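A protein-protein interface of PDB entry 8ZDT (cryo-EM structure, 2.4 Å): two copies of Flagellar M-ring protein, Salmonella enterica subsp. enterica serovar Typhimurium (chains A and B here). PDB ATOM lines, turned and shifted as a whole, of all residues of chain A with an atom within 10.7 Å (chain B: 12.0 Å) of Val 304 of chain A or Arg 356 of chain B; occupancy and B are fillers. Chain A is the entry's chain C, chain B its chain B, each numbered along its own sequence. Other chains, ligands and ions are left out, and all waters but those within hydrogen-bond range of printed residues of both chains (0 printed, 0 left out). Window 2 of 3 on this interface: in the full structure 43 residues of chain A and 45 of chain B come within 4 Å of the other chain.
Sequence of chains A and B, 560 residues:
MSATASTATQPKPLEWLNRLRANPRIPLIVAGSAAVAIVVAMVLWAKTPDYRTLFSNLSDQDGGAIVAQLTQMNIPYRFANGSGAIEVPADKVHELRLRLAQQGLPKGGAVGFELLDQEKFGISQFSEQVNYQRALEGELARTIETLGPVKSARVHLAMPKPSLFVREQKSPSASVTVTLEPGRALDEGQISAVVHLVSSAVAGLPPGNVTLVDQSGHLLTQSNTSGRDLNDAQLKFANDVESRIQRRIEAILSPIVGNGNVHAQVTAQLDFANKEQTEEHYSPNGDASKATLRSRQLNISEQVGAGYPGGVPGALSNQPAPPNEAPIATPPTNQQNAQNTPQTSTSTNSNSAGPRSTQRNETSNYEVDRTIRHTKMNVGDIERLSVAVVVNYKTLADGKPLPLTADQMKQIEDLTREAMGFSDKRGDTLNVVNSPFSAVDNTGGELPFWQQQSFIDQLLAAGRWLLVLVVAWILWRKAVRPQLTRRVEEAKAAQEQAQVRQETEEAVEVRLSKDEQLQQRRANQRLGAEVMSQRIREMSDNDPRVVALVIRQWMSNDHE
Ser 301 of chain A touches Thr 358 of chain B.
CG of Gln 359 of chain B touches OG of Ser 301 of chain A (3.5 Å).
O of Glu 302 of chain A touches O of Arg 356 of chain B, 3.98 Å away.
O of Glu 302 of chain A touches CA of Ser 357 of chain B, at 3.6 Å.
Gln 303 of chain A touches Arg 356 of chain B.
The backbone carbonyl oxygen (O) of Ser 301 of chain B sits at hydrogen-bond distance from the backbone NH (N) of Gln 359 of chain B (3.1 Å).
N of Ser 357 of chain B sits at hydrogen-bond distance from O of Gln 303 of chain B, at 2.9 Å.
The backbone carbonyl oxygen of Ser 301 of chain A lies within hydrogen-bond range of the backbone NH of Gln 359 of chain A (3.1 Å).
The backbone NH of Ser 357 of chain A sits at hydrogen-bond distance from the backbone carbonyl oxygen of Gln 303 of chain A (2.9 Å).
Of the printed residues of chain B, Ser 301 of chain A touches Thr 358 and Gln 359.
Glu 302 of chain A touches three residues of chain B.
Val 304 of chain A touches just one residue of chain B: Arg 356.
No residue of chain B comes within 4 Å of Pro 355 of chain A.
No residue of chain B comes within 4 Å of Arg 356 of chain A.
No residue of chain B comes within 4 Å of Ser 357 of chain A.
No residue of chain A comes within 4 Å of Pro 355 of chain B.
Of chain A, only Glu 302 (3.98 Å), Gln 303 (3.6 Å) and Val 304 (2.9 Å) come within 4 Å of Arg 356 of chain B.
Ser 357 of chain B touches just one residue of chain A: Glu 302 (3.6 Å).
Printed residues of chain A within 4 Å of Thr 358 of chain B: Ser 301 and Glu 302.
Printed residues of chain A within 4 Å of Gln 359 of chain B: Ser 301 (3.5 Å).
The nearest residue of chain A that does not touch Arg 356 of chain B is Pro 355 of chain A (7.2 Å).
Of the 9 printed residues of chain A, 4 touch a printed residue of chain B.
Printed residues of chain A that touch a printed residue of chain B: Ser 301, Glu 302, Gln 303 and Val 304.
Hydrophobic or aromatic side chains of chain A within 4 Å of the printed part of chain B: Val 304.
Among the printed residues, no Asp or Glu carboxylate lies within 4 Å of a Lys or Arg side-chain nitrogen of the other chain.
The backbone NH of Val 304 of chain A sits at hydrogen-bond distance from the backbone carbonyl oxygen of Arg 356 of chain B (2.9 Å).
The backbone NH (N) of Thr 358 of chain B is in hydrogen-bond range of the backbone carbonyl oxygen (O) of Glu 302 of chain A (3.1 Å).
Ser 301 of chain A touches Thr 358 of chain B, but with the chains exchanged Thr 358 of chain A does not touch Ser 301 of chain B (13.3 Å).
Glu 302 of chain A touches Arg 356 of chain B, but with the chains exchanged Arg 356 of chain A does not touch Glu 302 of chain B (15.7 Å).
Gln 303 of chain A touches Arg 356 of chain B, but with the chains exchanged Arg 356 of chain A does not touch Gln 303 of chain B (13.1 Å).
Val 304 of chain A touches Arg 356 of chain B, but with the chains exchanged Arg 356 of chain A does not touch Val 304 of chain B (14.5 Å).
9 positions are printed for both chains.
Of the 7 pairs that touch across the chains among the printed residues, none has its exchanged pair printed and touching as well.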
ATOM      1  N   SER A 301     -34.212 -23.509   1.906  1.00  0.00           N
ATOM      2  CA  SER A 301     -32.893 -23.480   2.521  1.00  0.00           C
ATOM      3  C   SER A 301     -32.964 -22.728   3.842  1.00  0.00           C
ATOM      4  O   SER A 301     -33.829 -21.871   4.038  1.00  0.00           O
ATOM      5  CB  SER A 301     -31.854 -22.821   1.606  1.00  0.00           C
ATOM      6  OG  SER A 301     -31.651 -23.584   0.431  1.00  0.00           O
ATOM      7  N   GLU A 302     -32.048 -23.059   4.748  1.00  0.00           N
ATOM      8  CA  GLU A 302     -32.019 -22.423   6.063  1.00  0.00           C
ATOM      9  C   GLU A 302     -30.641 -22.610   6.673  1.00  0.00           C
ATOM     10  O   GLU A 302     -30.170 -23.744   6.795  1.00  0.00           O
ATOM     11  CB  GLU A 302     -33.096 -23.010   6.972  1.00  0.00           C
ATOM     12  CG  GLU A 302     -32.971 -22.592   8.423  1.00  0.00           C
ATOM     13  CD  GLU A 302     -34.184 -22.982   9.241  1.00  0.00           C
ATOM     14  OE1 GLU A 302     -35.304 -22.959   8.691  1.00  0.00           O
ATOM     15  OE2 GLU A 302     -34.017 -23.312  10.435  1.00  0.00           O
ATOM     16  N   GLN A 303     -30.000 -21.508   7.056  1.00  0.00           N
ATOM     17  CA  GLN A 303     -28.703 -21.532   7.718  1.00  0.00           C
ATOM     18  C   GLN A 303     -28.822 -20.845   9.069  1.00  0.00           C
ATOM     19  O   GLN A 303     -29.347 -19.730   9.159  1.00  0.00           O
ATOM     20  CB  GLN A 303     -27.631 -20.844   6.869  1.00  0.00           C
ATOM     21  CG  GLN A 303     -27.299 -21.569   5.580  1.00  0.00           C
ATOM     22  CD  GLN A 303     -26.272 -20.831   4.746  1.00  0.00           C
ATOM     23  OE1 GLN A 303     -26.124 -19.614   4.857  1.00  0.00           O
ATOM     24  NE2 GLN A 303     -25.555 -21.564   3.904  1.00  0.00           N
ATOM     25  N   VAL A 304     -28.337 -21.507  10.114  1.00  0.00           N
ATOM     26  CA  VAL A 304     -28.390 -20.950  11.459  1.00  0.00           C
ATOM     27  C   VAL A 304     -27.003 -20.953  12.089  1.00  0.00           C
ATOM     28  O   VAL A 304     -26.045 -20.450  11.503  1.00  0.00           O
ATOM     29  CB  VAL A 304     -29.386 -21.719  12.342  1.00  0.00           C
ATOM     30  CG1 VAL A 304     -29.174 -21.368  13.804  1.00  0.00           C
ATOM     31  CG2 VAL A 304     -30.813 -21.415  11.919  1.00  0.00           C
ATOM     32  N   PRO A 355     -26.600 -15.128  13.209  1.00  0.00           N
ATOM     33  CA  PRO A 355     -26.926 -14.959  11.790  1.00  0.00           C
ATOM     34  C   PRO A 355     -27.907 -16.013  11.281  1.00  0.00           C
ATOM     35  O   PRO A 355     -27.530 -17.173  11.116  1.00  0.00           O
ATOM     36  CB  PRO A 355     -25.567 -15.103  11.103  1.00  0.00           C
ATOM     37  CG  PRO A 355     -24.591 -14.632  12.119  1.00  0.00           C
ATOM     38  CD  PRO A 355     -25.151 -15.029  13.460  1.00  0.00           C
ATOM     39  N   ARG A 356     -29.150 -15.607  11.039  1.00  0.00           N
ATOM     40  CA  ARG A 356     -30.196 -16.497  10.549  1.00  0.00           C
ATOM     41  C   ARG A 356     -30.484 -16.163   9.094  1.00  0.00           C
ATOM     42  O   ARG A 356     -30.670 -14.992   8.749  1.00  0.00           O
ATOM     43  CB  ARG A 356     -31.486 -16.377  11.374  1.00  0.00           C
ATOM     44  CG  ARG A 356     -31.519 -17.078  12.742  1.00  0.00           C
ATOM     45  CD  ARG A 356     -30.242 -16.934  13.558  1.00  0.00           C
ATOM     46  NE  ARG A 356     -30.101 -15.592  14.110  1.00  0.00           N
ATOM     47  CZ  ARG A 356     -29.187 -15.239  15.003  1.00  0.00           C
ATOM     48  NH1 ARG A 356     -28.309 -16.109  15.477  1.00  0.00           N
ATOM     49  NH2 ARG A 356     -29.150 -13.980  15.431  1.00  0.00           N
ATOM     50  N   SER A 357     -30.519 -17.188   8.245  1.00  0.00           N
ATOM     51  CA  SER A 357     -30.823 -17.028   6.830  1.00  0.00           C
ATOM     52  C   SER A 357     -31.914 -18.009   6.431  1.00  0.00           C
ATOM     53  O   SER A 357     -31.919 -19.160   6.875  1.00  0.00           O
ATOM     54  CB  SER A 357     -29.578 -17.247   5.962  1.00  0.00           C
ATOM     55  OG  SER A 357     -28.559 -16.320   6.290  1.00  0.00           O
ATOM     56  N   THR A 358     -32.842 -17.545   5.596  1.00  0.00           N
ATOM     57  CA  THR A 358     -33.955 -18.363   5.137  1.00  0.00           C
ATOM     58  C   THR A 358     -34.266 -18.031   3.685  1.00  0.00           C
ATOM     59  O   THR A 358     -34.236 -16.863   3.288  1.00  0.00           O
ATOM     60  CB  THR A 358     -35.205 -18.148   5.999  1.00  0.00           C
ATOM     61  OG1 THR A 358     -34.828 -18.077   7.380  1.00  0.00           O
ATOM     62  CG2 THR A 358     -36.189 -19.289   5.809  1.00  0.00           C
ATOM     63  N   GLN A 359     -34.558 -19.063   2.897  1.00  0.00           N
ATOM     64  CA  GLN A 359     -34.903 -18.901   1.493  1.00  0.00           C
ATOM     65  C   GLN A 359     -36.066 -19.819   1.149  1.00  0.00           C
ATOM     66  O   GLN A 359     -36.275 -20.849   1.794  1.00  0.00           O
ATOM     67  CB  GLN A 359     -33.709 -19.204   0.581  1.00  0.00           C
ATOM     68  CG  GLN A 359     -33.031 -17.971   0.022  1.00  0.00           C
ATOM     69  CD  GLN A 359     -31.798 -18.304  -0.789  1.00  0.00           C
ATOM     70  OE1 GLN A 359     -31.310 -19.433  -0.761  1.00  0.00           O
ATOM     71  NE2 GLN A 359     -31.285 -17.321  -1.519  1.00  0.00           N
ATOM     72  N   SER B 301     -30.324 -32.466   2.226  1.00  0.00           N
ATOM     73  CA  SER B 301     -28.989 -32.304   2.781  1.00  0.00           C
ATOM     74  C   SER B 301     -29.089 -31.713   4.180  1.00  0.00           C
ATOM     75  O   SER B 301     -30.054 -31.019   4.509  1.00  0.00           O
ATOM     76  CB  SER B 301     -28.112 -31.405   1.901  1.00  0.00           C
ATOM     77  OG  SER B 301     -27.873 -32.003   0.640  1.00  0.00           O
ATOM     78  N   GLU B 302     -28.081 -31.995   5.001  1.00  0.00           N
ATOM     79  CA  GLU B 302     -28.065 -31.503   6.377  1.00  0.00           C
ATOM     80  C   GLU B 302     -26.640 -31.545   6.901  1.00  0.00           C
ATOM     81  O   GLU B 302     -26.004 -32.602   6.874  1.00  0.00           O
ATOM     82  CB  GLU B 302     -28.989 -32.336   7.261  1.00  0.00           C
ATOM     83  CG  GLU B 302     -28.839 -32.057   8.743  1.00  0.00           C
ATOM     84  CD  GLU B 302     -29.932 -32.707   9.565  1.00  0.00           C
ATOM     85  OE1 GLU B 302     -31.075 -32.794   9.070  1.00  0.00           O
ATOM     86  OE2 GLU B 302     -29.648 -33.130  10.705  1.00  0.00           O
ATOM     87  N   GLN B 303     -26.142 -30.406   7.376  1.00  0.00           N
ATOM     88  CA  GLN B 303     -24.817 -30.304   7.973  1.00  0.00           C
ATOM     89  C   GLN B 303     -24.953 -29.786   9.397  1.00  0.00           C
ATOM     90  O   GLN B 303     -25.626 -28.779   9.633  1.00  0.00           O
ATOM     91  CB  GLN B 303     -23.910 -29.379   7.160  1.00  0.00           C
ATOM     92  CG  GLN B 303     -23.554 -29.908   5.785  1.00  0.00           C
ATOM     93  CD  GLN B 303     -22.695 -28.942   4.995  1.00  0.00           C
ATOM     94  OE1 GLN B 303     -22.718 -27.735   5.234  1.00  0.00           O
ATOM     95  NE2 GLN B 303     -21.932 -29.468   4.044  1.00  0.00           N
ATOM     96  N   VAL B 304     -24.315 -30.473  10.338  1.00  0.00           N
ATOM     97  CA  VAL B 304     -24.367 -30.074  11.739  1.00  0.00           C
ATOM     98  C   VAL B 304     -22.960 -29.936  12.302  1.00  0.00           C
ATOM     99  O   VAL B 304     -22.120 -29.238  11.735  1.00  0.00           O
ATOM    100  CB  VAL B 304     -25.188 -31.071  12.573  1.00  0.00           C
ATOM    101  CG1 VAL B 304     -24.941 -30.846  14.054  1.00  0.00           C
ATOM    102  CG2 VAL B 304     -26.667 -30.941  12.250  1.00  0.00           C
ATOM    103  N   PRO B 355     -23.330 -24.264  14.047  1.00  0.00           N
ATOM    104  CA  PRO B 355     -23.762 -23.999  12.672  1.00  0.00           C
ATOM    105  C   PRO B 355     -24.610 -25.129  12.092  1.00  0.00           C
ATOM    106  O   PRO B 355     -24.082 -26.196  11.783  1.00  0.00           O
ATOM    107  CB  PRO B 355     -22.441 -23.867  11.914  1.00  0.00           C
ATOM    108  CG  PRO B 355     -21.483 -23.363  12.932  1.00  0.00           C
ATOM    109  CD  PRO B 355     -21.898 -23.977  14.244  1.00  0.00           C
ATOM    110  N   ARG B 356     -25.911 -24.890  11.952  1.00  0.00           N
ATOM    111  CA  ARG B 356     -26.845 -25.870  11.413  1.00  0.00           C
ATOM    112  C   ARG B 356     -27.265 -25.433  10.018  1.00  0.00           C
ATOM    113  O   ARG B 356     -27.639 -24.274   9.815  1.00  0.00           O
ATOM    114  CB  ARG B 356     -28.088 -26.031  12.302  1.00  0.00           C
ATOM    115  CG  ARG B 356     -27.937 -26.868  13.583  1.00  0.00           C
ATOM    116  CD  ARG B 356     -26.648 -26.622  14.352  1.00  0.00           C
ATOM    117  NE  ARG B 356     -26.669 -25.338  15.045  1.00  0.00           N
ATOM    118  CZ  ARG B 356     -25.762 -24.947  15.930  1.00  0.00           C
ATOM    119  NH1 ARG B 356     -24.742 -25.720  16.265  1.00  0.00           N
ATOM    120  NH2 ARG B 356     -25.881 -23.748  16.495  1.00  0.00           N
ATOM    121  N   SER B 357     -27.204 -26.358   9.062  1.00  0.00           N
ATOM    122  CA  SER B 357     -27.612 -26.099   7.689  1.00  0.00           C
ATOM    123  C   SER B 357     -28.574 -27.184   7.231  1.00  0.00           C
ATOM    124  O   SER B 357     -28.386 -28.364   7.544  1.00  0.00           O
ATOM    125  CB  SER B 357     -26.403 -26.039   6.748  1.00  0.00           C
ATOM    126  OG  SER B 357     -25.509 -25.010   7.132  1.00  0.00           O
ATOM    127  N   THR B 358     -29.607 -26.781   6.494  1.00  0.00           N
ATOM    128  CA  THR B 358     -30.616 -27.703   5.997  1.00  0.00           C
ATOM    129  C   THR B 358     -31.058 -27.271   4.606  1.00  0.00           C
ATOM    130  O   THR B 358     -31.220 -26.078   4.341  1.00  0.00           O
ATOM    131  CB  THR B 358     -31.830 -27.768   6.932  1.00  0.00           C
ATOM    132  OG1 THR B 358     -31.385 -27.786   8.294  1.00  0.00           O
ATOM    133  CG2 THR B 358     -32.650 -29.017   6.659  1.00  0.00           C
ATOM    134  N   GLN B 359     -31.246 -28.249   3.721  1.00  0.00           N
ATOM    135  CA  GLN B 359     -31.694 -27.995   2.360  1.00  0.00           C
ATOM    136  C   GLN B 359     -32.732 -29.035   1.968  1.00  0.00           C
ATOM    137  O   GLN B 359     -32.751 -30.146   2.502  1.00  0.00           O
ATOM    138  CB  GLN B 359     -30.526 -28.020   1.369  1.00  0.00           C
ATOM    139  CG  GLN B 359     -30.067 -26.647   0.922  1.00  0.00           C
ATOM    140  CD  GLN B 359     -28.850 -26.706   0.025  1.00  0.00           C
ATOM    141  OE1 GLN B 359     -28.204 -27.746  -0.095  1.00  0.00           O
ATOM    142  NE2 GLN B 359     -28.529 -25.587  -0.612  1.00  0.00           N
ATOM    143  N   ARG B 360     -33.597 -28.663   1.026  1.00  0.00           N
ATOM    144  CA  ARG B 360     -34.624 -29.579   0.535  1.00  0.00           C
ATOM    145  C   ARG B 360     -35.109 -29.091  -0.819  1.00  0.00           C
ATOM    146  O   ARG B 360     -35.693 -28.007  -0.910  1.00  0.00           O
ATOM    147  CB  ARG B 360     -35.784 -29.678   1.521  1.00  0.00           C
ATOM    148  CG  ARG B 360     -36.664 -30.892   1.306  1.00  0.00           C
ATOM    149  CD  ARG B 360     -37.803 -30.939   2.304  1.00  0.00           C
ATOM    150  NE  ARG B 360     -39.004 -31.525   1.724  1.00  0.00           N
ATOM    151  CZ  ARG B 360     -39.425 -32.759   1.964  1.00  0.00           C
ATOM    152  NH1 ARG B 360     -38.766 -33.569   2.776  1.00  0.00           N
ATOM    153  NH2 ARG B 360     -40.535 -33.192   1.373  1.00  0.00           N
